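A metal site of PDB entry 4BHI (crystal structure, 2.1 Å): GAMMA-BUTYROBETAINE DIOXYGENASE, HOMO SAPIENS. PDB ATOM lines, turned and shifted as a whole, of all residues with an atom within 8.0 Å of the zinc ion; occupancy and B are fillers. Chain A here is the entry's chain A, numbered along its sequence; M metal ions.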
ATOM      1  N   LEU A  34      18.901 -13.460 -19.786  1.00  0.00           N
ATOM      2  CA  LEU A  34      17.967 -14.273 -19.008  1.00  0.00           C
ATOM      3  C   LEU A  34      18.381 -15.745 -18.980  1.00  0.00           C
ATOM      4  O   LEU A  34      18.429 -16.340 -17.938  1.00  0.00           O
ATOM      5  CB  LEU A  34      16.558 -14.162 -19.593  1.00  0.00           C
ATOM      6  CG  LEU A  34      15.843 -12.811 -19.436  1.00  0.00           C
ATOM      7  CD1 LEU A  34      14.663 -12.779 -20.387  1.00  0.00           C
ATOM      8  CD2 LEU A  34      15.383 -12.558 -18.015  1.00  0.00           C
ATOM      9  N   ARG A  35      18.681 -16.318 -20.129  1.00  0.00           N
ATOM     10  CA  ARG A  35      19.106 -17.724 -20.162  1.00  0.00           C
ATOM     11  C   ARG A  35      20.419 -17.961 -19.400  1.00  0.00           C
ATOM     12  O   ARG A  35      20.556 -18.949 -18.644  1.00  0.00           O
ATOM     13  CB  ARG A  35      19.239 -18.219 -21.601  1.00  0.00           C
ATOM     14  CG  ARG A  35      19.747 -19.660 -21.708  1.00  0.00           C
ATOM     15  CD  ARG A  35      18.644 -20.661 -21.344  1.00  0.00           C
ATOM     16  NE  ARG A  35      19.092 -22.049 -21.159  1.00  0.00           N
ATOM     17  CZ  ARG A  35      19.727 -22.515 -20.094  1.00  0.00           C
ATOM     18  NH1 ARG A  35      20.023 -21.714 -19.086  1.00  0.00           N
ATOM     19  NH2 ARG A  35      20.087 -23.823 -20.024  1.00  0.00           N
ATOM     20  N   ASP A  36      21.376 -17.039 -19.610  1.00  0.00           N
ATOM     21  CA  ASP A  36      22.667 -17.060 -18.908  1.00  0.00           C
ATOM     22  C   ASP A  36      22.445 -17.042 -17.401  1.00  0.00           C
ATOM     23  O   ASP A  36      23.193 -17.672 -16.629  1.00  0.00           O
ATOM     24  CB  ASP A  36      23.510 -15.823 -19.276  1.00  0.00           C
ATOM     25  CG  ASP A  36      24.845 -15.802 -18.553  1.00  0.00           C
ATOM     26  OD1 ASP A  36      25.566 -16.840 -18.589  1.00  0.00           O
ATOM     27  OD2 ASP A  36      25.171 -14.747 -17.968  1.00  0.00           O
ATOM     28  N   ASN A  37      21.392 -16.337 -16.990  1.00  0.00           N
ATOM     29  CA  ASN A  37      21.120 -16.179 -15.561  1.00  0.00           C
ATOM     30  C   ASN A  37      19.931 -16.927 -14.996  1.00  0.00           C
ATOM     31  O   ASN A  37      19.416 -16.577 -13.930  1.00  0.00           O
ATOM     32  CB  ASN A  37      21.082 -14.706 -15.240  1.00  0.00           C
ATOM     33  CG  ASN A  37      22.442 -14.084 -15.408  1.00  0.00           C
ATOM     34  OD1 ASN A  37      23.366 -14.428 -14.678  1.00  0.00           O
ATOM     35  ND2 ASN A  37      22.583 -13.220 -16.405  1.00  0.00           N
ATOM     36  N   CYS A  38      19.571 -18.020 -15.642  1.00  0.00           N
ATOM     37  CA  CYS A  38      18.585 -18.967 -15.091  1.00  0.00           C
ATOM     38  C   CYS A  38      18.980 -19.403 -13.695  1.00  0.00           C
ATOM     39  O   CYS A  38      20.083 -19.872 -13.479  1.00  0.00           O
ATOM     40  CB  CYS A  38      18.466 -20.209 -15.990  1.00  0.00           C
ATOM     41  SG  CYS A  38      17.237 -21.416 -15.388  1.00  0.00           S
ATOM     42  N   PRO A  39      18.063 -19.260 -12.716  1.00  0.00           N
ATOM     43  CA  PRO A  39      18.400 -19.664 -11.350  1.00  0.00           C
ATOM     44  C   PRO A  39      18.098 -21.113 -10.994  1.00  0.00           C
ATOM     45  O   PRO A  39      18.206 -21.487  -9.846  1.00  0.00           O
ATOM     46  CB  PRO A  39      17.567 -18.714 -10.497  1.00  0.00           C
ATOM     47  CG  PRO A  39      16.361 -18.392 -11.347  1.00  0.00           C
ATOM     48  CD  PRO A  39      16.813 -18.456 -12.789  1.00  0.00           C
ATOM     49  N   CYS A  40      17.721 -21.946 -11.965  1.00  0.00           N
ATOM     50  CA  CYS A  40      17.347 -23.313 -11.671  1.00  0.00           C
ATOM     51  C   CYS A  40      18.604 -24.056 -11.178  1.00  0.00           C
ATOM     52  O   CYS A  40      19.725 -23.572 -11.338  1.00  0.00           O
ATOM     53  CB  CYS A  40      16.749 -23.997 -12.924  1.00  0.00           C
ATOM     54  SG  CYS A  40      17.938 -24.909 -13.952  1.00  0.00           S
ATOM     55  N   SER A  41      18.409 -25.232 -10.601  1.00  0.00           N
ATOM     56  CA  SER A  41      19.495 -25.922  -9.922  1.00  0.00           C
ATOM     57  C   SER A  41      20.465 -26.559 -10.924  1.00  0.00           C
ATOM     58  O   SER A  41      21.570 -26.941 -10.550  1.00  0.00           O
ATOM     59  CB  SER A  41      18.940 -26.920  -8.887  1.00  0.00           C
ATOM     60  OG  SER A  41      18.636 -28.182  -9.454  1.00  0.00           O
ATOM     61  N   ASP A  42      20.064 -26.683 -12.197  1.00  0.00           N
ATOM     62  CA  ASP A  42      21.012 -27.082 -13.252  1.00  0.00           C
ATOM     63  C   ASP A  42      22.040 -25.975 -13.568  1.00  0.00           C
ATOM     64  O   ASP A  42      23.231 -26.256 -13.791  1.00  0.00           O
ATOM     65  CB  ASP A  42      20.273 -27.464 -14.529  1.00  0.00           C
ATOM     66  CG  ASP A  42      19.540 -28.781 -14.424  1.00  0.00           C
ATOM     67  OD1 ASP A  42      19.574 -29.461 -13.373  1.00  0.00           O
ATOM     68  OD2 ASP A  42      18.937 -29.156 -15.425  1.00  0.00           O
ATOM     69  N   CYS A  43      21.554 -24.739 -13.599  1.00  0.00           N
ATOM     70  CA  CYS A  43      22.304 -23.569 -14.058  1.00  0.00           C
ATOM     71  C   CYS A  43      22.991 -22.771 -12.979  1.00  0.00           C
ATOM     72  O   CYS A  43      23.865 -21.976 -13.266  1.00  0.00           O
ATOM     73  CB  CYS A  43      21.358 -22.620 -14.791  1.00  0.00           C
ATOM     74  SG  CYS A  43      20.613 -23.421 -16.197  1.00  0.00           S
ATOM     75  N   TYR A  44      22.600 -23.001 -11.728  1.00  0.00           N
ATOM     76  CA  TYR A  44      22.980 -22.114 -10.657  1.00  0.00           C
ATOM     77  C   TYR A  44      23.128 -22.894  -9.344  1.00  0.00           C
ATOM     78  O   TYR A  44      22.190 -23.582  -8.926  1.00  0.00           O
ATOM     79  CB  TYR A  44      21.921 -21.017 -10.528  1.00  0.00           C
ATOM     80  CG  TYR A  44      22.344 -19.878  -9.661  1.00  0.00           C
ATOM     81  CD1 TYR A  44      23.108 -18.848 -10.192  1.00  0.00           C
ATOM     82  CD2 TYR A  44      21.983 -19.818  -8.312  1.00  0.00           C
ATOM     83  CE1 TYR A  44      23.510 -17.789  -9.408  1.00  0.00           C
ATOM     84  CE2 TYR A  44      22.386 -18.755  -7.515  1.00  0.00           C
ATOM     85  CZ  TYR A  44      23.153 -17.747  -8.076  1.00  0.00           C
ATOM     86  OH  TYR A  44      23.589 -16.681  -7.334  1.00  0.00           O
ATOM     87  N   LEU A  53      26.173 -22.862 -15.215  1.00  0.00           N
ATOM     88  CA  LEU A  53      26.000 -22.845 -16.647  1.00  0.00           C
ATOM     89  C   LEU A  53      27.296 -22.437 -17.337  1.00  0.00           C
ATOM     90  O   LEU A  53      27.903 -21.434 -16.987  1.00  0.00           O
ATOM     91  CB  LEU A  53      24.868 -21.886 -17.014  1.00  0.00           C
ATOM     92  CG  LEU A  53      24.434 -21.868 -18.470  1.00  0.00           C
ATOM     93  CD1 LEU A  53      23.676 -23.129 -18.849  1.00  0.00           C
ATOM     94  CD2 LEU A  53      23.583 -20.650 -18.672  1.00  0.00           C
ATOM     95  N   TRP A  78      12.375 -22.308 -23.174  1.00  0.00           N
ATOM     96  CA  TRP A  78      13.386 -22.013 -24.155  1.00  0.00           C
ATOM     97  C   TRP A  78      13.304 -22.957 -25.356  1.00  0.00           C
ATOM     98  O   TRP A  78      12.687 -24.011 -25.289  1.00  0.00           O
ATOM     99  CB  TRP A  78      14.776 -22.073 -23.489  1.00  0.00           C
ATOM    100  CG  TRP A  78      14.990 -21.008 -22.421  1.00  0.00           C
ATOM    101  CD1 TRP A  78      15.066 -21.220 -21.065  1.00  0.00           C
ATOM    102  CD2 TRP A  78      15.193 -19.612 -22.618  1.00  0.00           C
ATOM    103  NE1 TRP A  78      15.289 -20.042 -20.412  1.00  0.00           N
ATOM    104  CE2 TRP A  78      15.374 -19.029 -21.339  1.00  0.00           C
ATOM    105  CE3 TRP A  78      15.250 -18.787 -23.739  1.00  0.00           C
ATOM    106  CZ2 TRP A  78      15.588 -17.660 -21.159  1.00  0.00           C
ATOM    107  CZ3 TRP A  78      15.475 -17.420 -23.567  1.00  0.00           C
ATOM    108  CH2 TRP A  78      15.633 -16.855 -22.280  1.00  0.00           C
ATOM    109  N   HIS A  82      14.513 -26.188 -22.228  1.00  0.00           N
ATOM    110  CA  HIS A  82      14.890 -25.698 -20.903  1.00  0.00           C
ATOM    111  C   HIS A  82      13.810 -24.739 -20.371  1.00  0.00           C
ATOM    112  O   HIS A  82      13.092 -24.038 -21.161  1.00  0.00           O
ATOM    113  CB  HIS A  82      16.295 -25.081 -20.921  1.00  0.00           C
ATOM    114  CG  HIS A  82      16.891 -24.917 -19.575  1.00  0.00           C
ATOM    115  ND1 HIS A  82      17.407 -25.961 -18.862  1.00  0.00           N
ATOM    116  CD2 HIS A  82      16.965 -23.841 -18.766  1.00  0.00           C
ATOM    117  CE1 HIS A  82      17.818 -25.531 -17.683  1.00  0.00           C
ATOM    118  NE2 HIS A  82      17.565 -24.241 -17.610  1.00  0.00           N
ATOM    119  N   TYR A  83      13.647 -24.728 -19.060  1.00  0.00           N
ATOM    120  CA  TYR A  83      12.598 -23.969 -18.390  1.00  0.00           C
ATOM    121  C   TYR A  83      13.189 -23.056 -17.324  1.00  0.00           C
ATOM    122  O   TYR A  83      13.987 -23.505 -16.521  1.00  0.00           O
ATOM    123  CB  TYR A  83      11.571 -24.950 -17.766  1.00  0.00           C
ATOM    124  CG  TYR A  83      10.565 -24.288 -16.891  1.00  0.00           C
ATOM    125  CD1 TYR A  83       9.621 -23.427 -17.420  1.00  0.00           C
ATOM    126  CD2 TYR A  83      10.549 -24.511 -15.505  1.00  0.00           C
ATOM    127  CE1 TYR A  83       8.687 -22.798 -16.612  1.00  0.00           C
ATOM    128  CE2 TYR A  83       9.636 -23.885 -14.690  1.00  0.00           C
ATOM    129  CZ  TYR A  83       8.694 -23.030 -15.254  1.00  0.00           C
ATOM    130  OH  TYR A  83       7.756 -22.405 -14.437  1.00  0.00           O
ATOM    131  N   SER A  84      12.810 -21.783 -17.313  1.00  0.00           N
ATOM    132  CA  SER A  84      13.303 -20.836 -16.314  1.00  0.00           C
ATOM    133  C   SER A  84      12.182 -19.997 -15.639  1.00  0.00           C
ATOM    134  O   SER A  84      11.211 -19.591 -16.283  1.00  0.00           O
ATOM    135  CB  SER A  84      14.354 -19.893 -16.933  1.00  0.00           C
ATOM    136  OG  SER A  84      15.406 -20.587 -17.611  1.00  0.00           O
ATOM    137  N   GLU A  85      12.371 -19.710 -14.346  1.00  0.00           N
ATOM    138  CA  GLU A  85      11.517 -18.804 -13.596  1.00  0.00           C
ATOM    139  C   GLU A  85      12.325 -17.637 -13.043  1.00  0.00           C
ATOM    140  O   GLU A  85      13.416 -17.833 -12.502  1.00  0.00           O
ATOM    141  CB  GLU A  85      10.849 -19.540 -12.445  1.00  0.00           C
ATOM    142  CG  GLU A  85      10.168 -20.839 -12.867  1.00  0.00           C
ATOM    143  CD  GLU A  85       9.287 -21.437 -11.785  1.00  0.00           C
ATOM    144  OE1 GLU A  85       9.432 -21.034 -10.621  1.00  0.00           O
ATOM    145  OE2 GLU A  85       8.477 -22.338 -12.101  1.00  0.00           O
ATOM    146  N   PHE A  86      11.789 -16.430 -13.159  1.00  0.00           N
ATOM    147  CA  PHE A  86      12.445 -15.230 -12.626  1.00  0.00           C
ATOM    148  C   PHE A  86      11.470 -14.452 -11.764  1.00  0.00           C
ATOM    149  O   PHE A  86      10.301 -14.248 -12.138  1.00  0.00           O
ATOM    150  CB  PHE A  86      12.928 -14.330 -13.780  1.00  0.00           C
ATOM    151  CG  PHE A  86      13.864 -15.010 -14.720  1.00  0.00           C
ATOM    152  CD1 PHE A  86      15.233 -15.032 -14.465  1.00  0.00           C
ATOM    153  CD2 PHE A  86      13.383 -15.621 -15.869  1.00  0.00           C
ATOM    154  CE1 PHE A  86      16.100 -15.654 -15.339  1.00  0.00           C
ATOM    155  CE2 PHE A  86      14.255 -16.256 -16.746  1.00  0.00           C
ATOM    156  CZ  PHE A  86      15.620 -16.281 -16.482  1.00  0.00           C
HETATM  157 ZN    ZN M   1      18.277 -23.397 -15.736  1.00  0.00          ZN
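O of Cys 43 sits at hydrogen-bond distance from N of Leu 53, 3.1 Å away. SG of Cys 40 lies close to N of Asp 42. The side-chain sulfur (SG) of Cys 38 sits close to the side-chain hydroxyl (OG) of Ser 84 (3.0 Å). The guanidinium group (NH1) of Arg 35 sits close to the side-chain sulfur (SG) of Cys 43, at 3.4 Å.
Of the 18 residues printed, 4 come within 4 Å of the zinc ion.
The zinc ion is bound by NE2 of His 82 (2.2 Å), SG of Cys 38 (2.3 Å), SG of Cys 40 (2.4 Å) and SG of Cys 43 (2.4 Å).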
